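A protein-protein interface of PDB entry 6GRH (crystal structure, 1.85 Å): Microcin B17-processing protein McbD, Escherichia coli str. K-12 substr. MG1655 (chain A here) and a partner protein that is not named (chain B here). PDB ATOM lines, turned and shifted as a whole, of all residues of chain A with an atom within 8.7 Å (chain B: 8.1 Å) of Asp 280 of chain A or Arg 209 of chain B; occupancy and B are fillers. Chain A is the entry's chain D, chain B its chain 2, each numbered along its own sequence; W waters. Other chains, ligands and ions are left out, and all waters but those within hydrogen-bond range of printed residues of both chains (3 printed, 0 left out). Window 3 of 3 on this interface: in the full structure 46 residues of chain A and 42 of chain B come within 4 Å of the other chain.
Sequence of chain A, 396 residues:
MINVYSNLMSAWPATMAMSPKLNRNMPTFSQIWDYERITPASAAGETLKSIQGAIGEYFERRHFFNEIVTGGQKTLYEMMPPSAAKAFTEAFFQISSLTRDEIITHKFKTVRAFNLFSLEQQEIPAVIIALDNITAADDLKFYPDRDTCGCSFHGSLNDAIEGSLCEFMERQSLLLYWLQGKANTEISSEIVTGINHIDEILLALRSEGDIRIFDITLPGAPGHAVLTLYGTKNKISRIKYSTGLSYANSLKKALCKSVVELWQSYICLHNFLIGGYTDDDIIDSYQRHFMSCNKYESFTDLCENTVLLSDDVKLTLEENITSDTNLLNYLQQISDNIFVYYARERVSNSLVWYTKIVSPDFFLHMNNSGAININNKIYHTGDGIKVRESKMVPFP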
ATOM      1  N   ASP A  34      14.032  -8.651  12.068  1.00  0.00           N
ATOM      2  CA  ASP A  34      14.668  -9.938  12.290  1.00  0.00           C
ATOM      3  C   ASP A  34      13.751 -10.784  13.186  1.00  0.00           C
ATOM      4  O   ASP A  34      14.155 -11.191  14.264  1.00  0.00           O
ATOM      5  CB  ASP A  34      16.054  -9.728  12.928  1.00  0.00           C
ATOM      6  CG  ASP A  34      17.018 -10.895  12.693  1.00  0.00           C
ATOM      7  OD1 ASP A  34      16.735 -11.755  11.814  1.00  0.00           O
ATOM      8  OD2 ASP A  34      18.080 -10.941  13.397  1.00  0.00           O
ATOM      9  N   TYR A  35      12.532 -11.051  12.715  1.00  0.00           N
ATOM     10  CA  TYR A  35      11.570 -11.911  13.422  1.00  0.00           C
ATOM     11  C   TYR A  35      11.376 -11.308  14.821  1.00  0.00           C
ATOM     12  O   TYR A  35      11.275 -10.088  14.931  1.00  0.00           O
ATOM     13  CB  TYR A  35      12.052 -13.377  13.456  1.00  0.00           C
ATOM     14  CG  TYR A  35      12.412 -13.903  12.086  1.00  0.00           C
ATOM     15  CD1 TYR A  35      11.418 -14.297  11.194  1.00  0.00           C
ATOM     16  CD2 TYR A  35      13.742 -13.996  11.683  1.00  0.00           C
ATOM     17  CE1 TYR A  35      11.747 -14.766   9.923  1.00  0.00           C
ATOM     18  CE2 TYR A  35      14.086 -14.463  10.428  1.00  0.00           C
ATOM     19  CZ  TYR A  35      13.088 -14.842   9.554  1.00  0.00           C
ATOM     20  OH  TYR A  35      13.433 -15.291   8.318  1.00  0.00           O
ATOM     21  N   GLU A  36      11.428 -12.120  15.868  1.00  0.00           N
ATOM     22  CA  GLU A  36      11.388 -11.611  17.224  1.00  0.00           C
ATOM     23  C   GLU A  36      12.667 -11.966  17.954  1.00  0.00           C
ATOM     24  O   GLU A  36      12.695 -12.047  19.196  1.00  0.00           O
ATOM     25  CB  GLU A  36      10.140 -12.135  17.919  1.00  0.00           C
ATOM     26  CG  GLU A  36       8.869 -11.707  17.198  1.00  0.00           C
ATOM     27  CD  GLU A  36       7.595 -12.189  17.868  1.00  0.00           C
ATOM     28  OE1 GLU A  36       7.508 -13.332  18.363  1.00  0.00           O
ATOM     29  OE2 GLU A  36       6.648 -11.397  17.890  1.00  0.00           O
ATOM     30  N   ARG A  37      13.757 -12.106  17.189  1.00  0.00           N
ATOM     31  CA  ARG A  37      15.065 -12.262  17.791  1.00  0.00           C
ATOM     32  C   ARG A  37      15.391 -10.999  18.605  1.00  0.00           C
ATOM     33  O   ARG A  37      15.862 -11.107  19.731  1.00  0.00           O
ATOM     34  CB  ARG A  37      16.120 -12.522  16.732  1.00  0.00           C
ATOM     35  CG  ARG A  37      15.999 -13.872  16.064  1.00  0.00           C
ATOM     36  CD  ARG A  37      16.537 -13.830  14.627  1.00  0.00           C
ATOM     37  NE  ARG A  37      16.598 -15.167  14.041  1.00  0.00           N
ATOM     38  CZ  ARG A  37      16.978 -15.425  12.790  1.00  0.00           C
ATOM     39  NH1 ARG A  37      17.321 -14.426  11.961  1.00  0.00           N
ATOM     40  NH2 ARG A  37      16.996 -16.682  12.353  1.00  0.00           N
ATOM     41  N   ILE A  38      15.117  -9.840  18.003  1.00  0.00           N
ATOM     42  CA  ILE A  38      15.100  -8.506  18.654  1.00  0.00           C
ATOM     43  C   ILE A  38      13.898  -7.749  18.104  1.00  0.00           C
ATOM     44  O   ILE A  38      13.303  -8.182  17.113  1.00  0.00           O
ATOM     45  CB  ILE A  38      16.377  -7.698  18.393  1.00  0.00           C
ATOM     46  CG1 ILE A  38      16.653  -7.563  16.891  1.00  0.00           C
ATOM     47  CG2 ILE A  38      17.563  -8.343  19.088  1.00  0.00           C
ATOM     48  CD1 ILE A  38      17.735  -6.563  16.539  1.00  0.00           C
ATOM     49  N   THR A  39      13.527  -6.627  18.702  1.00  0.00           N
ATOM     50  CA  THR A  39      12.481  -5.802  18.093  1.00  0.00           C
ATOM     51  C   THR A  39      13.129  -5.054  16.902  1.00  0.00           C
ATOM     52  O   THR A  39      14.334  -4.868  16.889  1.00  0.00           O
ATOM     53  CB  THR A  39      11.887  -4.794  19.078  1.00  0.00           C
ATOM     54  OG1 THR A  39      12.932  -3.955  19.565  1.00  0.00           O
ATOM     55  CG2 THR A  39      11.204  -5.499  20.249  1.00  0.00           C
ATOM     56  N   PHE A  65      21.159  -8.179  23.397  1.00  0.00           N
ATOM     57  CA  PHE A  65      20.002  -9.092  23.581  1.00  0.00           C
ATOM     58  C   PHE A  65      20.288 -10.571  23.315  1.00  0.00           C
ATOM     59  O   PHE A  65      19.699 -11.452  23.961  1.00  0.00           O
ATOM     60  CB  PHE A  65      18.805  -8.654  22.711  1.00  0.00           C
ATOM     61  CG  PHE A  65      18.009  -7.521  23.285  1.00  0.00           C
ATOM     62  CD1 PHE A  65      18.434  -6.199  23.156  1.00  0.00           C
ATOM     63  CD2 PHE A  65      16.821  -7.776  23.957  1.00  0.00           C
ATOM     64  CE1 PHE A  65      17.695  -5.164  23.690  1.00  0.00           C
ATOM     65  CE2 PHE A  65      16.087  -6.736  24.519  1.00  0.00           C
ATOM     66  CZ  PHE A  65      16.521  -5.440  24.388  1.00  0.00           C
ATOM     67  N   ASN A  66      21.164 -10.875  22.364  1.00  0.00           N
ATOM     68  CA  ASN A  66      21.206 -12.248  21.820  1.00  0.00           C
ATOM     69  C   ASN A  66      22.542 -12.928  21.902  1.00  0.00           C
ATOM     70  O   ASN A  66      22.588 -14.146  21.636  1.00  0.00           O
ATOM     71  CB  ASN A  66      20.869 -12.280  20.331  1.00  0.00           C
ATOM     72  CG  ASN A  66      19.497 -11.757  19.990  1.00  0.00           C
ATOM     73  OD1 ASN A  66      19.317 -11.282  18.869  1.00  0.00           O
ATOM     74  ND2 ASN A  66      18.535 -11.840  20.898  1.00  0.00           N
ATOM     75  N   PHE A 272       2.355   1.650  13.484  1.00  0.00           N
ATOM     76  CA  PHE A 272       1.831   0.561  14.310  1.00  0.00           C
ATOM     77  C   PHE A 272       0.297   0.707  14.457  1.00  0.00           C
ATOM     78  O   PHE A 272      -0.463  -0.248  14.182  1.00  0.00           O
ATOM     79  CB  PHE A 272       2.543   0.547  15.676  1.00  0.00           C
ATOM     80  CG  PHE A 272       2.150  -0.606  16.545  1.00  0.00           C
ATOM     81  CD1 PHE A 272       1.008  -0.539  17.329  1.00  0.00           C
ATOM     82  CD2 PHE A 272       2.892  -1.785  16.527  1.00  0.00           C
ATOM     83  CE1 PHE A 272       0.620  -1.627  18.112  1.00  0.00           C
ATOM     84  CE2 PHE A 272       2.509  -2.871  17.310  1.00  0.00           C
ATOM     85  CZ  PHE A 272       1.373  -2.793  18.095  1.00  0.00           C
ATOM     86  N   TYR A 277      -2.039  -3.396  14.292  1.00  0.00           N
ATOM     87  CA  TYR A 277      -1.287  -4.459  14.970  1.00  0.00           C
ATOM     88  C   TYR A 277      -1.774  -4.618  16.422  1.00  0.00           C
ATOM     89  O   TYR A 277      -2.094  -3.631  17.088  1.00  0.00           O
ATOM     90  CB  TYR A 277       0.212  -4.156  14.944  1.00  0.00           C
ATOM     91  CG  TYR A 277       0.808  -4.178  13.549  1.00  0.00           C
ATOM     92  CD1 TYR A 277       1.114  -5.384  12.910  1.00  0.00           C
ATOM     93  CD2 TYR A 277       1.050  -2.986  12.857  1.00  0.00           C
ATOM     94  CE1 TYR A 277       1.655  -5.399  11.626  1.00  0.00           C
ATOM     95  CE2 TYR A 277       1.586  -2.986  11.580  1.00  0.00           C
ATOM     96  CZ  TYR A 277       1.892  -4.187  10.965  1.00  0.00           C
ATOM     97  OH  TYR A 277       2.425  -4.158   9.689  1.00  0.00           O
ATOM     98  N   THR A 278      -1.829  -5.860  16.896  1.00  0.00           N
ATOM     99  CA  THR A 278      -2.373  -6.162  18.228  1.00  0.00           C
ATOM    100  C   THR A 278      -1.307  -5.945  19.293  1.00  0.00           C
ATOM    101  O   THR A 278      -0.117  -5.782  18.986  1.00  0.00           O
ATOM    102  CB  THR A 278      -2.854  -7.626  18.328  1.00  0.00           C
ATOM    103  OG1 THR A 278      -1.740  -8.512  18.168  1.00  0.00           O
ATOM    104  CG2 THR A 278      -3.879  -7.936  17.253  1.00  0.00           C
ATOM    105  N   ASP A 279      -1.743  -5.979  20.547  1.00  0.00           N
ATOM    106  CA  ASP A 279      -0.828  -5.911  21.687  1.00  0.00           C
ATOM    107  C   ASP A 279       0.088  -7.135  21.809  1.00  0.00           C
ATOM    108  O   ASP A 279       1.192  -7.013  22.347  1.00  0.00           O
ATOM    109  CB  ASP A 279      -1.593  -5.673  23.002  1.00  0.00           C
ATOM    110  CG  ASP A 279      -1.850  -4.186  23.276  1.00  0.00           C
ATOM    111  OD1 ASP A 279      -1.465  -3.324  22.452  1.00  0.00           O
ATOM    112  OD2 ASP A 279      -2.434  -3.880  24.338  1.00  0.00           O
ATOM    113  N   ASP A 280      -0.338  -8.290  21.287  1.00  0.00           N
ATOM    114  CA  ASP A 280       0.542  -9.459  21.252  1.00  0.00           C
ATOM    115  C   ASP A 280       1.773  -9.275  20.336  1.00  0.00           C
ATOM    116  O   ASP A 280       2.737 -10.036  20.434  1.00  0.00           O
ATOM    117  CB  ASP A 280      -0.225 -10.720  20.855  1.00  0.00           C
ATOM    118  CG  ASP A 280       0.603 -11.985  21.067  1.00  0.00           C
ATOM    119  OD1 ASP A 280       0.913 -12.316  22.240  1.00  0.00           O
ATOM    120  OD2 ASP A 280       0.979 -12.622  20.064  1.00  0.00           O
ATOM    121  N   ASP A 281       1.736  -8.277  19.450  1.00  0.00           N
ATOM    122  CA  ASP A 281       2.885  -7.932  18.614  1.00  0.00           C
ATOM    123  C   ASP A 281       3.924  -7.109  19.364  1.00  0.00           C
ATOM    124  O   ASP A 281       5.049  -7.001  18.904  1.00  0.00           O
ATOM    125  CB  ASP A 281       2.438  -7.166  17.367  1.00  0.00           C
ATOM    126  CG  ASP A 281       1.466  -7.958  16.519  1.00  0.00           C
ATOM    127  OD1 ASP A 281       1.641  -9.180  16.435  1.00  0.00           O
ATOM    128  OD2 ASP A 281       0.514  -7.369  15.962  1.00  0.00           O
ATOM    129  N   ILE A 282       3.541  -6.512  20.491  1.00  0.00           N
ATOM    130  CA  ILE A 282       4.474  -5.761  21.322  1.00  0.00           C
ATOM    131  C   ILE A 282       5.096  -6.720  22.320  1.00  0.00           C
ATOM    132  O   ILE A 282       4.383  -7.264  23.169  1.00  0.00           O
ATOM    133  CB  ILE A 282       3.780  -4.600  22.061  1.00  0.00           C
ATOM    134  CG1 ILE A 282       3.146  -3.623  21.058  1.00  0.00           C
ATOM    135  CG2 ILE A 282       4.776  -3.861  22.958  1.00  0.00           C
ATOM    136  CD1 ILE A 282       4.139  -3.024  20.062  1.00  0.00           C
ATOM    137  N   ILE A 283       6.404  -6.942  22.195  1.00  0.00           N
ATOM    138  CA  ILE A 283       7.140  -7.834  23.108  1.00  0.00           C
ATOM    139  C   ILE A 283       8.052  -7.117  24.105  1.00  0.00           C
ATOM    140  O   ILE A 283       8.613  -7.781  24.973  1.00  0.00           O
ATOM    141  CB  ILE A 283       7.975  -8.897  22.348  1.00  0.00           C
ATOM    142  CG1 ILE A 283       9.141  -8.271  21.580  1.00  0.00           C
ATOM    143  CG2 ILE A 283       7.064  -9.710  21.436  1.00  0.00           C
ATOM    144  CD1 ILE A 283       9.974  -9.267  20.799  1.00  0.00           C
ATOM    145  N   ASP A 284       8.223  -5.795  23.956  1.00  0.00           N
ATOM    146  CA  ASP A 284       9.138  -5.015  24.785  1.00  0.00           C
ATOM    147  C   ASP A 284       8.356  -4.190  25.821  1.00  0.00           C
ATOM    148  O   ASP A 284       7.473  -3.405  25.466  1.00  0.00           O
ATOM    149  CB  ASP A 284       9.956  -4.092  23.873  1.00  0.00           C
ATOM    150  CG  ASP A 284      11.022  -3.308  24.613  1.00  0.00           C
ATOM    151  OD1 ASP A 284      10.684  -2.547  25.520  1.00  0.00           O
ATOM    152  OD2 ASP A 284      12.205  -3.422  24.271  1.00  0.00           O
ATOM    153  N   ARG A 288       5.714  -1.102  25.352  1.00  0.00           N
ATOM    154  CA  ARG A 288       4.348  -1.225  25.893  1.00  0.00           C
ATOM    155  C   ARG A 288       4.018  -0.046  26.809  1.00  0.00           C
ATOM    156  O   ARG A 288       2.972   0.577  26.679  1.00  0.00           O
ATOM    157  CB  ARG A 288       4.157  -2.566  26.643  1.00  0.00           C
ATOM    158  CG  ARG A 288       2.705  -2.929  26.970  1.00  0.00           C
ATOM    159  CD  ARG A 288       2.548  -4.317  27.602  1.00  0.00           C
ATOM    160  NE  ARG A 288       3.123  -5.353  26.745  1.00  0.00           N
ATOM    161  CZ  ARG A 288       4.253  -6.047  26.962  1.00  0.00           C
ATOM    162  NH1 ARG A 288       4.982  -5.935  28.086  1.00  0.00           N
ATOM    163  NH2 ARG A 288       4.634  -6.931  26.042  1.00  0.00           N
ATOM    164  N   ARG B 203      21.500 -16.825  18.935  1.00  0.00           N
ATOM    165  CA  ARG B 203      20.474 -15.847  18.622  1.00  0.00           C
ATOM    166  C   ARG B 203      19.057 -16.460  18.723  1.00  0.00           C
ATOM    167  O   ARG B 203      18.110 -15.787  19.195  1.00  0.00           O
ATOM    168  CB  ARG B 203      20.773 -15.178  17.259  1.00  0.00           C
ATOM    169  CG  ARG B 203      19.792 -14.095  16.834  1.00  0.00           C
ATOM    170  CD  ARG B 203      20.095 -13.475  15.451  1.00  0.00           C
ATOM    171  NE  ARG B 203      20.090 -14.475  14.379  1.00  0.00           N
ATOM    172  CZ  ARG B 203      20.407 -14.222  13.110  1.00  0.00           C
ATOM    173  NH1 ARG B 203      20.690 -12.966  12.700  1.00  0.00           N
ATOM    174  NH2 ARG B 203      20.431 -15.214  12.236  1.00  0.00           N
ATOM    175  N   GLU B 204      18.919 -17.742  18.357  1.00  0.00           N
ATOM    176  CA  GLU B 204      17.644 -18.449  18.554  1.00  0.00           C
ATOM    177  C   GLU B 204      17.335 -18.665  20.056  1.00  0.00           C
ATOM    178  O   GLU B 204      16.249 -18.312  20.535  1.00  0.00           O
ATOM    179  CB  GLU B 204      17.632 -19.790  17.798  1.00  0.00           C
ATOM    180  CG  GLU B 204      17.741 -19.687  16.285  1.00  0.00           C
ATOM    181  CD  GLU B 204      16.607 -18.876  15.662  1.00  0.00           C
ATOM    182  OE1 GLU B 204      15.433 -19.307  15.758  1.00  0.00           O
ATOM    183  OE2 GLU B 204      16.888 -17.793  15.107  1.00  0.00           O
ATOM    184  N   GLU B 205      18.316 -19.196  20.783  1.00  0.00           N
ATOM    185  CA  GLU B 205      18.188 -19.517  22.222  1.00  0.00           C
ATOM    186  C   GLU B 205      17.905 -18.246  23.041  1.00  0.00           C
ATOM    187  O   GLU B 205      17.029 -18.216  23.929  1.00  0.00           O
ATOM    188  CB  GLU B 205      19.488 -20.179  22.702  1.00  0.00           C
ATOM    189  CG  GLU B 205      19.542 -20.593  24.182  1.00  0.00           C
ATOM    190  CD  GLU B 205      20.965 -20.817  24.751  1.00  0.00           C
ATOM    191  OE1 GLU B 205      21.992 -20.334  24.169  1.00  0.00           O
ATOM    192  OE2 GLU B 205      21.051 -21.464  25.845  1.00  0.00           O
ATOM    193  N   LYS B 206      18.625 -17.177  22.695  1.00  0.00           N
ATOM    194  CA  LYS B 206      18.505 -15.919  23.410  1.00  0.00           C
ATOM    195  C   LYS B 206      17.569 -14.903  22.724  1.00  0.00           C
ATOM    196  O   LYS B 206      17.620 -13.715  23.026  1.00  0.00           O
ATOM    197  CB  LYS B 206      19.903 -15.367  23.663  1.00  0.00           C
ATOM    198  CG  LYS B 206      20.654 -16.158  24.718  1.00  0.00           C
ATOM    199  CD  LYS B 206      22.161 -15.895  24.781  1.00  0.00           C
ATOM    200  CE  LYS B 206      22.765 -16.538  26.037  1.00  0.00           C
ATOM    201  NZ  LYS B 206      24.215 -16.205  26.221  1.00  0.00           N
ATOM    202  N   SER B 207      16.695 -15.370  21.836  1.00  0.00           N
ATOM    203  CA  SER B 207      15.706 -14.495  21.191  1.00  0.00           C
ATOM    204  C   SER B 207      14.875 -13.765  22.231  1.00  0.00           C
ATOM    205  O   SER B 207      14.554 -14.332  23.284  1.00  0.00           O
ATOM    206  CB  SER B 207      14.774 -15.276  20.263  1.00  0.00           C
ATOM    207  OG  SER B 207      15.425 -15.570  19.040  1.00  0.00           O
ATOM    208  N   PHE B 208      14.506 -12.528  21.909  1.00  0.00           N
ATOM    209  CA  PHE B 208      13.725 -11.708  22.786  1.00  0.00           C
ATOM    210  C   PHE B 208      12.386 -12.411  23.044  1.00  0.00           C
ATOM    211  O   PHE B 208      11.934 -12.479  24.173  1.00  0.00           O
ATOM    212  CB  PHE B 208      13.470 -10.318  22.175  1.00  0.00           C
ATOM    213  CG  PHE B 208      13.084  -9.254  23.165  1.00  0.00           C
ATOM    214  CD1 PHE B 208      12.903  -9.506  24.544  1.00  0.00           C
ATOM    215  CD2 PHE B 208      12.926  -7.951  22.724  1.00  0.00           C
ATOM    216  CE1 PHE B 208      12.555  -8.484  25.421  1.00  0.00           C
ATOM    217  CE2 PHE B 208      12.596  -6.925  23.605  1.00  0.00           C
ATOM    218  CZ  PHE B 208      12.394  -7.192  24.949  1.00  0.00           C
ATOM    219  N   ARG B 209      11.762 -12.873  21.970  1.00  0.00           N
ATOM    220  CA  ARG B 209      10.690 -13.856  22.059  1.00  0.00           C
ATOM    221  C   ARG B 209      11.050 -15.059  21.226  1.00  0.00           C
ATOM    222  O   ARG B 209      11.086 -14.985  20.005  1.00  0.00           O
ATOM    223  CB  ARG B 209       9.316 -13.300  21.637  1.00  0.00           C
ATOM    224  CG  ARG B 209       8.208 -14.339  21.813  1.00  0.00           C
ATOM    225  CD  ARG B 209       6.851 -13.743  22.143  1.00  0.00           C
ATOM    226  NE  ARG B 209       6.195 -13.195  20.965  1.00  0.00           N
ATOM    227  CZ  ARG B 209       5.043 -12.516  20.995  1.00  0.00           C
ATOM    228  NH1 ARG B 209       4.401 -12.321  22.130  1.00  0.00           N
ATOM    229  NH2 ARG B 209       4.511 -12.051  19.864  1.00  0.00           N
ATOM    230  N   ARG B 210      11.348 -16.166  21.893  1.00  0.00           N
ATOM    231  CA  ARG B 210      11.738 -17.387  21.211  1.00  0.00           C
ATOM    232  C   ARG B 210      10.658 -17.844  20.266  1.00  0.00           C
ATOM    233  O   ARG B 210       9.486 -17.794  20.580  1.00  0.00           O
ATOM    234  CB  ARG B 210      11.925 -18.534  22.180  1.00  0.00           C
ATOM    235  CG  ARG B 210      13.173 -18.493  23.018  1.00  0.00           C
ATOM    236  CD  ARG B 210      13.301 -19.822  23.769  1.00  0.00           C
ATOM    237  NE  ARG B 210      14.641 -19.922  24.316  1.00  0.00           N
ATOM    238  CZ  ARG B 210      15.257 -21.040  24.668  1.00  0.00           C
ATOM    239  NH1 ARG B 210      14.661 -22.239  24.566  1.00  0.00           N
ATOM    240  NH2 ARG B 210      16.494 -20.950  25.144  1.00  0.00           N
ATOM    241  N   ASN B 211      11.088 -18.288  19.103  1.00  0.00           N
ATOM    242  CA  ASN B 211      10.234 -19.021  18.207  1.00  0.00           C
ATOM    243  C   ASN B 211      10.271 -20.493  18.705  1.00  0.00           C
ATOM    244  O   ASN B 211      11.284 -21.193  18.559  1.00  0.00           O
ATOM    245  CB  ASN B 211      10.759 -18.857  16.784  1.00  0.00           C
ATOM    246  CG  ASN B 211      10.021 -19.708  15.770  1.00  0.00           C
ATOM    247  OD1 ASN B 211       8.989 -20.319  16.067  1.00  0.00           O
ATOM    248  ND2 ASN B 211      10.541 -19.727  14.542  1.00  0.00           N
ATOM    249  N   GLU B 212       9.163 -20.935  19.279  1.00  0.00           N
ATOM    250  CA  GLU B 212       8.986 -22.321  19.716  1.00  0.00           C
ATOM    251  C   GLU B 212       9.138 -23.356  18.580  1.00  0.00           C
ATOM    252  O   GLU B 212       9.383 -24.520  18.866  1.00  0.00           O
ATOM    253  CB  GLU B 212       7.603 -22.494  20.361  1.00  0.00           C
HETATM  254  O   HOH W   1      11.575 -15.049  16.561  1.00  0.00           O
HETATM  255  O   HOH W   2      16.911 -11.540  24.431  1.00  0.00           O
HETATM  256  O   HOH W   3      19.546 -17.182  14.635  1.00  0.00           O
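Water W2 bridges the backbone carbonyl oxygen of Lys 206 of chain B (2.7 Å) and the backbone carbonyl oxygen of Phe 65 of chain A (2.8 Å).
Water W3 lies within hydrogen-bond range of the side-chain carboxylate (OE2) of Glu 204 of chain B (2.8 Å), the guanidinium group (NE) of Arg 203 of chain B (2.8 Å) and the guanidinium group (NH2) of Arg 37 of chain A (3.5 Å).
Water W1 lies within hydrogen-bond range of the backbone NH (N) of Glu 36 of chain A and the backbone carbonyl oxygen (O) of Arg 209 of chain B.
The backbone NH (N) of Asp 280 of chain A sits close to the side-chain hydroxyl (OG1) of Thr 278 of chain A (3.4 Å).
O of Arg 37 of chain A sits at hydrogen-bond distance from ND2 of Asn 66 of chain A (3.0 Å).
The backbone carbonyl oxygen (O) of Arg 203 of chain B sits at hydrogen-bond distance from the side-chain hydroxyl (OG) of Ser 207 of chain B (2.7 Å).
The backbone carbonyl oxygen (O) of Glu 204 of chain B is in hydrogen-bond range of the side-chain hydroxyl (OG) of Ser 207 of chain B (3.2 Å).
NH1 of Arg 37 of chain A lies within salt-bridge range of OD1 of Asp 34 of chain A (2.7 Å).
O of Glu 36 of chain A touches CB of Ser 207 of chain B (3.99 Å).
OG of Ser 207 of chain B touches CG of Arg 37 of chain A, at 3.5 Å.
CD2 of Phe 208 of chain B touches CG2 of Thr 39 of chain A (3.9 Å).
Phe 65 of chain A touches Phe 208 of chain B.
Arg 203 of chain B touches Asn 66 of chain A.
Ser 207 of chain B touches Asn 66 of chain A (CA to ND2, 3.9 Å).
Ile 283 of chain A touches Phe 208 of chain B (CD1 to CD2, 3.8 Å).
Arg 209 of chain B touches Ile 283 of chain A.
Asp 284 of chain A touches Phe 208 of chain B.
The backbone NH (N) of Phe 208 of chain B is in hydrogen-bond range of the backbone carbonyl oxygen (O) of Arg 37 of chain A (2.9 Å).
NE of Arg 209 of chain B lies within salt-bridge range of OE1 of Glu 36 of chain A (2.9 Å).
The guanidinium group (NH1) of Arg 37 of chain A sits close to the guanidinium group (NH2) of Arg 203 of chain B (3.2 Å).
The guanidinium group of Arg 203 of chain B is in salt-bridge range of the side-chain carboxylate of Asp 34 of chain A (3.4 Å).
O of Lys 206 of chain B is in hydrogen-bond range of ND2 of Asn 66 of chain A.
The guanidinium group (NH1) of Arg 209 of chain B lies within salt-bridge range of the side-chain carboxylate (OD1) of Asp 280 of chain A (3.5 Å).
O of Lys 206 of chain B sits close to O of Phe 65 of chain A (3.2 Å).
OE2 of Glu 204 of chain B lies within salt-bridge range of NE of Arg 37 of chain A (2.8 Å).
N of Phe 208 of chain B lies within hydrogen-bond range of O of Glu 36 of chain A.
Of chain B, only Arg 209 comes within 4 Å of Asp 280 of chain A.
Ile 282 of chain A touches none of the printed residues of chain B.
Of the printed residues of chain B, Asp 284 of chain A touches Phe 208.
Printed residues of chain A within 4 Å of Arg 203 of chain B: Asp 34 (3.4 Å), Arg 37 (3.2 Å) and Asn 66 (3.5 Å).
Of the printed residues of chain A, Glu 204 of chain B touches Arg 37 (2.8 Å).
Of the printed residues of chain A, Lys 206 of chain B touches Phe 65 and Asn 66.
Of chain A, only Glu 36 (2.9 Å), Asp 280 (2.7 Å) and Ile 283 (3.5 Å) come within 4 Å of Arg 209 of chain B.
Glu 212 of chain B touches none of the printed residues of chain A.
Hydrophobic or aromatic side chains of chain A that line the printed part of chain B: Phe 65 and Ile 283.
Among the printed residues, 18 pairs touch across the chains.
Among the printed residues, Asp or Glu carboxylates within 4 Å of a Lys or Arg side-chain nitrogen of the other chain: Asp 34 of chain A with Arg 203 of chain B, Glu 36 of chain A with Arg 209 of chain B, Arg 37 of chain A with Glu 204 of chain B and Asp 280 of chain A with Arg 209 of chain B.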
